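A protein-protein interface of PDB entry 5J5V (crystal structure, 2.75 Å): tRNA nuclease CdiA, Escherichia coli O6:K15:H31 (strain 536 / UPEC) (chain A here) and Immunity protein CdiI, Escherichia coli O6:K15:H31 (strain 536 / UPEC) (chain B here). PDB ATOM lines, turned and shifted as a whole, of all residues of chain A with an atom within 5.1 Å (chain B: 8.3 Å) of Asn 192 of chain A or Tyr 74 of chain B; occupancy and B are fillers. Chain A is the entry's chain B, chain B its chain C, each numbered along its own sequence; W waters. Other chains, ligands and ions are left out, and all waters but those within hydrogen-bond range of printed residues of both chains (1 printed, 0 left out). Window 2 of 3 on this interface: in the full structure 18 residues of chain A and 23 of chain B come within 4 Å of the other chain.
Asn 185 of chain A touches Arg 48 of chain B. Tyr 73 of chain B touches Asn 185 of chain A (CD2 to ND2, 3.5 Å). NE of Arg 188 of chain A touches CE2 of Tyr 74 of chain B (3.5 Å). Arg 188 of chain A touches Ala 80 of chain B (NH1 to CB, 3.9 Å). NH2 of Arg 188 of chain A touches CG2 of Ile 112 of chain B, 3.6 Å away. CA of Asn 113 of chain B touches NH2 of Arg 188 of chain A, 3.9 Å away. Arg 188 of chain A touches Leu 116 of chain B (NH2 to CD1, 3.0 Å). Tyr 73 of chain B touches Gly 189 of chain A. Tyr 74 of chain B touches Gly 189 of chain A (CD1 to CA, 3.6 Å). His 193 of chain A touches Tyr 74 of chain B.
Of the 11 printed residues of chain A, 5 touch a printed residue of chain B. Hydrophobic or aromatic side chains of chain A within 4 Å of the printed part of chain B: His 193. Hydrophobic or aromatic side chains of chain B within 4 Å of the printed part of chain A: Tyr 73, Tyr 74, Ala 80, Ile 112 and Leu 116.
OE2 of Glu 77 of chain B lies close to SG of Cys 44 of chain B (3.6 Å). The side-chain carboxylate of Glu 77 of chain B lies within salt-bridge range of the guanidinium group of Arg 48 of chain B. The backbone NH (N) of Glu 77 of chain B is in hydrogen-bond range of the backbone carbonyl oxygen (O) of Ala 70 of chain B, at 3.4 Å. The backbone NH of Glu 72 of chain B sits at hydrogen-bond distance from the side-chain carboxylate of Glu 77 of chain B, 2.9 Å away. The side-chain carboxylate (OE1) of Glu 77 of chain B sits at hydrogen-bond distance from the backbone NH (N) of Tyr 73 of chain B (2.9 Å). The backbone NH (N) of Asn 113 of chain B sits close to the side-chain carboxylate (OD1) of Asp 111 of chain B (3.1 Å).
Asn 192 of chain A touches just one residue of chain B: Tyr 74. Of the printed residues of chain A, Glu 77 of chain B touches Asn 185 (3.3 Å). Of the printed residues of chain A, Leu 116 of chain B touches Arg 188. Of the printed residues of chain A, Ile 112 of chain B touches Arg 188 (3.6 Å). Leu 78 of chain B touches none of the printed residues of chain A. Thr 196 of chain A touches none of the printed residues of chain B. The nearest residue of chain B that does not touch Asn 192 of chain A is Asp 75 of chain B (4.6 Å).
The side-chain hydroxyl (OH) of Tyr 74 of chain B lies within hydrogen-bond range of the side-chain amide oxygen (OD1) of Asn 185 of chain A (2.7 Å). OE2 of Glu 77 of chain B sits at hydrogen-bond distance from ND2 of Asn 185 of chain A, 3.3 Å away. O of Tyr 73 of chain B sits at hydrogen-bond distance from NE2 of His 193 of chain A, 2.7 Å away.
Water W1 lies within hydrogen-bond range of the guanidinium group of Arg 48 of chain B (3.0 Å), the backbone carbonyl oxygen of Glu 77 of chain B (3.1 Å), the backbone NH of Ala 81 of chain B (3.2 Å), the side-chain amide oxygen of Asn 185 of chain A (3.3 Å) and the side-chain hydroxyl of Tyr 74 of chain B (3.4 Å).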
ATOM      1  N   ASN A 185      -7.800  15.577 -22.391  1.00  0.00           N
ATOM      2  CA  ASN A 185      -7.565  14.435 -23.256  1.00  0.00           C
ATOM      3  C   ASN A 185      -8.742  14.218 -24.191  1.00  0.00           C
ATOM      4  O   ASN A 185      -8.558  13.893 -25.367  1.00  0.00           O
ATOM      5  CB  ASN A 185      -7.317  13.196 -22.407  1.00  0.00           C
ATOM      6  CG  ASN A 185      -6.786  12.045 -23.212  1.00  0.00           C
ATOM      7  OD1 ASN A 185      -5.688  12.104 -23.746  1.00  0.00           O
ATOM      8  ND2 ASN A 185      -7.564  10.990 -23.308  1.00  0.00           N
ATOM      9  N   LEU A 187     -10.971  16.494 -25.212  1.00  0.00           N
ATOM     10  CA  LEU A 187     -10.922  17.547 -26.212  1.00  0.00           C
ATOM     11  C   LEU A 187      -9.911  17.209 -27.290  1.00  0.00           C
ATOM     12  O   LEU A 187     -10.159  17.432 -28.481  1.00  0.00           O
ATOM     13  CB  LEU A 187     -10.572  18.875 -25.550  1.00  0.00           C
ATOM     14  CG  LEU A 187     -11.711  19.802 -25.102  1.00  0.00           C
ATOM     15  CD1 LEU A 187     -11.132  21.020 -24.458  1.00  0.00           C
ATOM     16  CD2 LEU A 187     -12.620  20.201 -26.248  1.00  0.00           C
ATOM     17  N   ARG A 188      -8.763  16.669 -26.895  1.00  0.00           N
ATOM     18  CA  ARG A 188      -7.716  16.419 -27.869  1.00  0.00           C
ATOM     19  C   ARG A 188      -8.141  15.351 -28.861  1.00  0.00           C
ATOM     20  O   ARG A 188      -7.941  15.506 -30.067  1.00  0.00           O
ATOM     21  CB  ARG A 188      -6.425  16.033 -27.159  1.00  0.00           C
ATOM     22  CG  ARG A 188      -5.323  15.695 -28.090  1.00  0.00           C
ATOM     23  CD  ARG A 188      -4.024  15.608 -27.374  1.00  0.00           C
ATOM     24  NE  ARG A 188      -2.992  15.118 -28.275  1.00  0.00           N
ATOM     25  CZ  ARG A 188      -1.697  15.109 -28.008  1.00  0.00           C
ATOM     26  NH1 ARG A 188      -1.250  15.562 -26.851  1.00  0.00           N
ATOM     27  NH2 ARG A 188      -0.861  14.630 -28.905  1.00  0.00           N
ATOM     28  N   GLY A 189      -8.769  14.282 -28.383  1.00  0.00           N
ATOM     29  CA  GLY A 189      -9.240  13.258 -29.294  1.00  0.00           C
ATOM     30  C   GLY A 189     -10.301  13.779 -30.239  1.00  0.00           C
ATOM     31  O   GLY A 189     -10.224  13.572 -31.446  1.00  0.00           O
ATOM     32  N   LEU A 190     -11.315  14.454 -29.696  1.00  0.00           N
ATOM     33  CA  LEU A 190     -12.368  15.018 -30.533  1.00  0.00           C
ATOM     34  C   LEU A 190     -11.815  16.017 -31.535  1.00  0.00           C
ATOM     35  O   LEU A 190     -12.196  16.000 -32.708  1.00  0.00           O
ATOM     36  CB  LEU A 190     -13.429  15.688 -29.665  1.00  0.00           C
ATOM     37  CG  LEU A 190     -14.359  14.781 -28.877  1.00  0.00           C
ATOM     38  CD1 LEU A 190     -15.209  15.591 -27.943  1.00  0.00           C
ATOM     39  CD2 LEU A 190     -15.230  13.993 -29.838  1.00  0.00           C
ATOM     40  N   ARG A 191     -10.923  16.902 -31.089  1.00  0.00           N
ATOM     41  CA  ARG A 191     -10.342  17.872 -32.010  1.00  0.00           C
ATOM     42  C   ARG A 191      -9.550  17.178 -33.101  1.00  0.00           C
ATOM     43  O   ARG A 191      -9.601  17.580 -34.266  1.00  0.00           O
ATOM     44  CB  ARG A 191      -9.453  18.859 -31.257  1.00  0.00           C
ATOM     45  CG  ARG A 191     -10.220  20.010 -30.676  1.00  0.00           C
ATOM     46  CD  ARG A 191      -9.386  20.882 -29.775  1.00  0.00           C
ATOM     47  NE  ARG A 191     -10.169  22.025 -29.326  1.00  0.00           N
ATOM     48  CZ  ARG A 191      -9.985  22.634 -28.169  1.00  0.00           C
ATOM     49  NH1 ARG A 191      -9.041  22.213 -27.351  1.00  0.00           N
ATOM     50  NH2 ARG A 191     -10.741  23.660 -27.828  1.00  0.00           N
ATOM     51  N   ASN A 192      -8.834  16.116 -32.742  1.00  0.00           N
ATOM     52  CA  ASN A 192      -8.009  15.424 -33.715  1.00  0.00           C
ATOM     53  C   ASN A 192      -8.878  14.711 -34.742  1.00  0.00           C
ATOM     54  O   ASN A 192      -8.664  14.849 -35.949  1.00  0.00           O
ATOM     55  CB  ASN A 192      -7.087  14.454 -32.977  1.00  0.00           C
ATOM     56  CG  ASN A 192      -6.375  13.491 -33.888  1.00  0.00           C
ATOM     57  OD1 ASN A 192      -6.293  13.712 -35.098  1.00  0.00           O
ATOM     58  ND2 ASN A 192      -5.792  12.436 -33.299  1.00  0.00           N
ATOM     59  N   HIS A 193      -9.926  14.028 -34.291  1.00  0.00           N
ATOM     60  CA  HIS A 193     -10.782  13.279 -35.205  1.00  0.00           C
ATOM     61  C   HIS A 193     -11.632  14.189 -36.070  1.00  0.00           C
ATOM     62  O   HIS A 193     -12.004  13.815 -37.184  1.00  0.00           O
ATOM     63  CB  HIS A 193     -11.671  12.329 -34.420  1.00  0.00           C
ATOM     64  CG  HIS A 193     -10.921  11.275 -33.676  1.00  0.00           C
ATOM     65  ND1 HIS A 193      -9.929  10.520 -34.257  1.00  0.00           N
ATOM     66  CD2 HIS A 193     -11.006  10.857 -32.395  1.00  0.00           C
ATOM     67  CE1 HIS A 193      -9.438   9.679 -33.369  1.00  0.00           C
ATOM     68  NE2 HIS A 193     -10.068   9.870 -32.228  1.00  0.00           N
ATOM     69  N   ALA A 194     -11.995  15.356 -35.567  1.00  0.00           N
ATOM     70  CA  ALA A 194     -12.723  16.291 -36.402  1.00  0.00           C
ATOM     71  C   ALA A 194     -11.839  16.828 -37.515  1.00  0.00           C
ATOM     72  O   ALA A 194     -12.319  17.096 -38.618  1.00  0.00           O
ATOM     73  CB  ALA A 194     -13.285  17.419 -35.546  1.00  0.00           C
ATOM     74  N   ASP A 195     -10.546  17.005 -37.239  1.00  0.00           N
ATOM     75  CA  ASP A 195      -9.614  17.417 -38.282  1.00  0.00           C
ATOM     76  C   ASP A 195      -9.490  16.346 -39.346  1.00  0.00           C
ATOM     77  O   ASP A 195      -9.496  16.646 -40.545  1.00  0.00           O
ATOM     78  CB  ASP A 195      -8.245  17.740 -37.687  1.00  0.00           C
ATOM     79  CG  ASP A 195      -8.188  19.112 -37.055  1.00  0.00           C
ATOM     80  OD1 ASP A 195      -9.117  19.916 -37.266  1.00  0.00           O
ATOM     81  OD2 ASP A 195      -7.192  19.397 -36.363  1.00  0.00           O
ATOM     82  N   THR A 196      -9.350  15.087 -38.922  1.00  0.00           N
ATOM     83  CA  THR A 196      -9.302  13.976 -39.866  1.00  0.00           C
ATOM     84  C   THR A 196     -10.433  14.069 -40.875  1.00  0.00           C
ATOM     85  O   THR A 196     -10.223  13.869 -42.075  1.00  0.00           O
ATOM     86  CB  THR A 196      -9.387  12.641 -39.130  1.00  0.00           C
ATOM     87  OG1 THR A 196      -8.273  12.480 -38.250  1.00  0.00           O
ATOM     88  CG2 THR A 196      -9.403  11.504 -40.118  1.00  0.00           C
ATOM     89  N   VAL B  40      -5.724  -0.429 -22.912  1.00  0.00           N
ATOM     90  CA  VAL B  40      -4.915   0.724 -23.286  1.00  0.00           C
ATOM     91  C   VAL B  40      -5.484   1.984 -22.652  1.00  0.00           C
ATOM     92  O   VAL B  40      -4.743   2.824 -22.127  1.00  0.00           O
ATOM     93  CB  VAL B  40      -4.823   0.843 -24.813  1.00  0.00           C
ATOM     94  CG1 VAL B  40      -4.014   2.047 -25.174  1.00  0.00           C
ATOM     95  CG2 VAL B  40      -4.201  -0.398 -25.394  1.00  0.00           C
ATOM     96  N   CYS B  44      -3.232   4.505 -20.150  1.00  0.00           N
ATOM     97  CA  CYS B  44      -3.001   5.935 -20.313  1.00  0.00           C
ATOM     98  C   CYS B  44      -3.461   6.714 -19.093  1.00  0.00           C
ATOM     99  O   CYS B  44      -2.763   7.611 -18.610  1.00  0.00           O
ATOM    100  CB  CYS B  44      -3.737   6.453 -21.537  1.00  0.00           C
ATOM    101  SG  CYS B  44      -3.211   5.767 -23.030  1.00  0.00           S
ATOM    102  N   ARG B  48      -1.407   9.321 -16.632  1.00  0.00           N
ATOM    103  CA  ARG B  48      -1.905  10.682 -16.447  1.00  0.00           C
ATOM    104  C   ARG B  48      -2.206  11.011 -14.993  1.00  0.00           C
ATOM    105  O   ARG B  48      -1.990  12.137 -14.545  1.00  0.00           O
ATOM    106  CB  ARG B  48      -3.165  10.906 -17.281  1.00  0.00           C
ATOM    107  CG  ARG B  48      -2.887  11.092 -18.748  1.00  0.00           C
ATOM    108  CD  ARG B  48      -4.032  11.764 -19.472  1.00  0.00           C
ATOM    109  NE  ARG B  48      -5.255  10.980 -19.401  1.00  0.00           N
ATOM    110  CZ  ARG B  48      -5.561   9.986 -20.224  1.00  0.00           C
ATOM    111  NH1 ARG B  48      -4.724   9.646 -21.188  1.00  0.00           N
ATOM    112  NH2 ARG B  48      -6.704   9.330 -20.076  1.00  0.00           N
ATOM    113  N   GLU B  67       2.485  -1.747 -31.208  1.00  0.00           N
ATOM    114  CA  GLU B  67       1.691  -0.663 -31.764  1.00  0.00           C
ATOM    115  C   GLU B  67       2.204   0.634 -31.166  1.00  0.00           C
ATOM    116  O   GLU B  67       1.820   1.008 -30.053  1.00  0.00           O
ATOM    117  CB  GLU B  67       0.206  -0.862 -31.458  1.00  0.00           C
ATOM    118  CG  GLU B  67      -0.726   0.026 -32.248  1.00  0.00           C
ATOM    119  CD  GLU B  67      -2.186  -0.338 -32.032  1.00  0.00           C
ATOM    120  OE1 GLU B  67      -2.452  -1.367 -31.373  1.00  0.00           O
ATOM    121  OE2 GLU B  67      -3.072   0.408 -32.513  1.00  0.00           O
ATOM    122  N   LEU B  69       1.704   3.753 -31.809  1.00  0.00           N
ATOM    123  CA  LEU B  69       0.729   4.804 -31.556  1.00  0.00           C
ATOM    124  C   LEU B  69      -0.505   4.244 -30.866  1.00  0.00           C
ATOM    125  O   LEU B  69      -1.637   4.544 -31.255  1.00  0.00           O
ATOM    126  CB  LEU B  69       0.341   5.508 -32.853  1.00  0.00           C
ATOM    127  CG  LEU B  69       1.511   5.938 -33.733  1.00  0.00           C
ATOM    128  CD1 LEU B  69       1.064   6.019 -35.186  1.00  0.00           C
ATOM    129  CD2 LEU B  69       2.117   7.244 -33.260  1.00  0.00           C
ATOM    130  N   ALA B  70      -0.298   3.421 -29.847  1.00  0.00           N
ATOM    131  CA  ALA B  70      -1.424   2.893 -29.099  1.00  0.00           C
ATOM    132  C   ALA B  70      -2.187   4.030 -28.437  1.00  0.00           C
ATOM    133  O   ALA B  70      -1.602   5.004 -27.963  1.00  0.00           O
ATOM    134  CB  ALA B  70      -0.946   1.891 -28.057  1.00  0.00           C
ATOM    135  N   GLY B  71      -3.502   3.912 -28.441  1.00  0.00           N
ATOM    136  CA  GLY B  71      -4.339   4.878 -27.778  1.00  0.00           C
ATOM    137  C   GLY B  71      -5.787   4.516 -28.000  1.00  0.00           C
ATOM    138  O   GLY B  71      -6.138   3.839 -28.969  1.00  0.00           O
ATOM    139  N   GLU B  72      -6.622   5.002 -27.089  1.00  0.00           N
ATOM    140  CA  GLU B  72      -8.065   4.813 -27.147  1.00  0.00           C
ATOM    141  C   GLU B  72      -8.772   6.020 -27.756  1.00  0.00           C
ATOM    142  O   GLU B  72      -9.572   5.881 -28.684  1.00  0.00           O
ATOM    143  CB  GLU B  72      -8.594   4.528 -25.741  1.00  0.00           C
ATOM    144  CG  GLU B  72     -10.074   4.293 -25.681  1.00  0.00           C
ATOM    145  CD  GLU B  72     -10.502   3.156 -26.559  1.00  0.00           C
ATOM    146  OE1 GLU B  72      -9.812   2.120 -26.562  1.00  0.00           O
ATOM    147  OE2 GLU B  72     -11.529   3.293 -27.246  1.00  0.00           O
ATOM    148  N   TYR B  73      -8.531   7.204 -27.204  1.00  0.00           N
ATOM    149  CA  TYR B  73      -9.209   8.405 -27.662  1.00  0.00           C
ATOM    150  C   TYR B  73      -8.597   8.976 -28.923  1.00  0.00           C
ATOM    151  O   TYR B  73      -9.286   9.668 -29.673  1.00  0.00           O
ATOM    152  CB  TYR B  73      -9.189   9.449 -26.549  1.00  0.00           C
ATOM    153  CG  TYR B  73     -10.012   8.998 -25.385  1.00  0.00           C
ATOM    154  CD1 TYR B  73     -11.379   9.241 -25.347  1.00  0.00           C
ATOM    155  CD2 TYR B  73      -9.446   8.270 -24.358  1.00  0.00           C
ATOM    156  CE1 TYR B  73     -12.152   8.801 -24.300  1.00  0.00           C
ATOM    157  CE2 TYR B  73     -10.209   7.827 -23.301  1.00  0.00           C
ATOM    158  CZ  TYR B  73     -11.562   8.096 -23.280  1.00  0.00           C
ATOM    159  OH  TYR B  73     -12.327   7.656 -22.237  1.00  0.00           O
ATOM    160  N   TYR B  74      -7.328   8.696 -29.167  1.00  0.00           N
ATOM    161  CA  TYR B  74      -6.636   9.132 -30.361  1.00  0.00           C
ATOM    162  C   TYR B  74      -5.348   8.343 -30.450  1.00  0.00           C
ATOM    163  O   TYR B  74      -4.875   7.786 -29.458  1.00  0.00           O
ATOM    164  CB  TYR B  74      -6.363  10.634 -30.340  1.00  0.00           C
ATOM    165  CG  TYR B  74      -5.673  11.134 -29.092  1.00  0.00           C
ATOM    166  CD1 TYR B  74      -6.408  11.484 -27.974  1.00  0.00           C
ATOM    167  CD2 TYR B  74      -4.301  11.281 -29.037  1.00  0.00           C
ATOM    168  CE1 TYR B  74      -5.800  11.949 -26.837  1.00  0.00           C
ATOM    169  CE2 TYR B  74      -3.682  11.751 -27.895  1.00  0.00           C
ATOM    170  CZ  TYR B  74      -4.440  12.083 -26.800  1.00  0.00           C
ATOM    171  OH  TYR B  74      -3.849  12.550 -25.658  1.00  0.00           O
ATOM    172  N   ASP B  75      -4.786   8.310 -31.650  1.00  0.00           N
ATOM    173  CA  ASP B  75      -3.524   7.629 -31.866  1.00  0.00           C
ATOM    174  C   ASP B  75      -2.401   8.449 -31.262  1.00  0.00           C
ATOM    175  O   ASP B  75      -2.356   9.671 -31.411  1.00  0.00           O
ATOM    176  CB  ASP B  75      -3.292   7.416 -33.362  1.00  0.00           C
ATOM    177  CG  ASP B  75      -4.291   6.460 -33.972  1.00  0.00           C
ATOM    178  OD1 ASP B  75      -4.768   5.565 -33.245  1.00  0.00           O
ATOM    179  OD2 ASP B  75      -4.612   6.613 -35.166  1.00  0.00           O
ATOM    180  N   GLY B  76      -1.501   7.775 -30.559  1.00  0.00           N
ATOM    181  CA  GLY B  76      -0.448   8.448 -29.840  1.00  0.00           C
ATOM    182  C   GLY B  76      -0.782   8.822 -28.416  1.00  0.00           C
ATOM    183  O   GLY B  76       0.020   9.508 -27.775  1.00  0.00           O
ATOM    184  N   GLU B  77      -1.938   8.400 -27.905  1.00  0.00           N
ATOM    185  CA  GLU B  77      -2.367   8.812 -26.574  1.00  0.00           C
ATOM    186  C   GLU B  77      -1.417   8.312 -25.499  1.00  0.00           C
ATOM    187  O   GLU B  77      -1.176   9.004 -24.504  1.00  0.00           O
ATOM    188  CB  GLU B  77      -3.783   8.312 -26.299  1.00  0.00           C
ATOM    189  CG  GLU B  77      -4.280   8.622 -24.903  1.00  0.00           C
ATOM    190  CD  GLU B  77      -5.611   7.984 -24.612  1.00  0.00           C
ATOM    191  OE1 GLU B  77      -6.196   7.399 -25.530  1.00  0.00           O
ATOM    192  OE2 GLU B  77      -6.049   8.015 -23.453  1.00  0.00           O
ATOM    193  N   LEU B  78      -0.886   7.105 -25.668  1.00  0.00           N
ATOM    194  CA  LEU B  78       0.029   6.563 -24.675  1.00  0.00           C
ATOM    195  C   LEU B  78       1.305   7.393 -24.594  1.00  0.00           C
ATOM    196  O   LEU B  78       1.802   7.682 -23.501  1.00  0.00           O
ATOM    197  CB  LEU B  78       0.344   5.106 -25.010  1.00  0.00           C
ATOM    198  CG  LEU B  78       1.159   4.289 -24.008  1.00  0.00           C
ATOM    199  CD1 LEU B  78       0.651   4.494 -22.589  1.00  0.00           C
ATOM    200  CD2 LEU B  78       1.137   2.819 -24.381  1.00  0.00           C
ATOM    201  N   ILE B  79       1.841   7.799 -25.741  1.00  0.00           N
ATOM    202  CA  ILE B  79       2.986   8.702 -25.743  1.00  0.00           C
ATOM    203  C   ILE B  79       2.613  10.030 -25.105  1.00  0.00           C
ATOM    204  O   ILE B  79       3.393  10.618 -24.349  1.00  0.00           O
ATOM    205  CB  ILE B  79       3.502   8.883 -27.181  1.00  0.00           C
ATOM    206  CG1 ILE B  79       4.048   7.552 -27.713  1.00  0.00           C
ATOM    207  CG2 ILE B  79       4.538   9.977 -27.236  1.00  0.00           C
ATOM    208  CD1 ILE B  79       4.274   7.518 -29.194  1.00  0.00           C
ATOM    209  N   ALA B  80       1.409  10.519 -25.394  1.00  0.00           N
ATOM    210  CA  ALA B  80       0.933  11.740 -24.761  1.00  0.00           C
ATOM    211  C   ALA B  80       0.893  11.598 -23.245  1.00  0.00           C
ATOM    212  O   ALA B  80       1.314  12.502 -22.521  1.00  0.00           O
ATOM    213  CB  ALA B  80      -0.441  12.093 -25.314  1.00  0.00           C
ATOM    214  N   ALA B  81       0.390  10.471 -22.745  1.00  0.00           N
ATOM    215  CA  ALA B  81       0.368  10.254 -21.305  1.00  0.00           C
ATOM    216  C   ALA B  81       1.777  10.209 -20.731  1.00  0.00           C
ATOM    217  O   ALA B  81       2.051  10.824 -19.693  1.00  0.00           O
ATOM    218  CB  ALA B  81      -0.368   8.959 -20.982  1.00  0.00           C
ATOM    219  N   THR B  84       3.731  13.178 -19.547  1.00  0.00           N
ATOM    220  CA  THR B  84       3.361  13.820 -18.292  1.00  0.00           C
ATOM    221  C   THR B  84       4.146  13.293 -17.104  1.00  0.00           C
ATOM    222  O   THR B  84       3.936  13.754 -15.980  1.00  0.00           O
ATOM    223  CB  THR B  84       1.860  13.639 -18.040  1.00  0.00           C
ATOM    224  OG1 THR B  84       1.576  12.249 -17.861  1.00  0.00           O
ATOM    225  CG2 THR B  84       1.076  14.131 -19.227  1.00  0.00           C
ATOM    226  N   ASP B 111       2.525  14.937 -35.270  1.00  0.00           N
ATOM    227  CA  ASP B 111       2.107  16.328 -35.390  1.00  0.00           C
ATOM    228  C   ASP B 111       2.214  16.996 -34.033  1.00  0.00           C
ATOM    229  O   ASP B 111       3.298  17.056 -33.454  1.00  0.00           O
ATOM    230  CB  ASP B 111       0.672  16.416 -35.911  1.00  0.00           C
ATOM    231  CG  ASP B 111      -0.286  15.535 -35.135  1.00  0.00           C
ATOM    232  OD1 ASP B 111      -0.070  15.348 -33.919  1.00  0.00           O
ATOM    233  OD2 ASP B 111      -1.255  15.030 -35.739  1.00  0.00           O
ATOM    234  N   ILE B 112       1.095  17.489 -33.509  1.00  0.00           N
ATOM    235  CA  ILE B 112       1.129  18.022 -32.151  1.00  0.00           C
ATOM    236  C   ILE B 112       1.686  17.032 -31.143  1.00  0.00           C
ATOM    237  O   ILE B 112       1.973  17.406 -30.001  1.00  0.00           O
ATOM    238  CB  ILE B 112      -0.322  18.431 -31.812  1.00  0.00           C
ATOM    239  CG1 ILE B 112      -0.412  19.561 -30.792  1.00  0.00           C
ATOM    240  CG2 ILE B 112      -1.125  17.236 -31.323  1.00  0.00           C
ATOM    241  CD1 ILE B 112      -1.847  19.892 -30.436  1.00  0.00           C
ATOM    242  N   ASN B 113       1.833  15.769 -31.551  1.00  0.00           N
ATOM    243  CA  ASN B 113       2.580  14.749 -30.823  1.00  0.00           C
ATOM    244  C   ASN B 113       4.082  15.028 -30.770  1.00  0.00           C
ATOM    245  O   ASN B 113       4.748  14.606 -29.818  1.00  0.00           O
ATOM    246  CB  ASN B 113       2.282  13.394 -31.471  1.00  0.00           C
ATOM    247  CG  ASN B 113       2.648  12.218 -30.592  1.00  0.00           C
ATOM    248  OD1 ASN B 113       2.601  12.303 -29.364  1.00  0.00           O
ATOM    249  ND2 ASN B 113       2.938  11.082 -31.221  1.00  0.00           N
ATOM    250  N   LEU B 116       5.190  16.480 -27.616  1.00  0.00           N
ATOM    251  CA  LEU B 116       5.174  15.511 -26.533  1.00  0.00           C
ATOM    252  C   LEU B 116       6.416  14.653 -26.584  1.00  0.00           C
ATOM    253  O   LEU B 116       7.090  14.465 -25.566  1.00  0.00           O
ATOM    254  CB  LEU B 116       3.926  14.648 -26.592  1.00  0.00           C
ATOM    255  CG  LEU B 116       2.625  15.416 -26.690  1.00  0.00           C
ATOM    256  CD1 LEU B 116       1.614  14.420 -27.155  1.00  0.00           C
ATOM    257  CD2 LEU B 116       2.244  16.048 -25.362  1.00  0.00           C
HETATM  258  O   HOH W   1      -2.714  11.092 -22.828  1.00  0.00           O
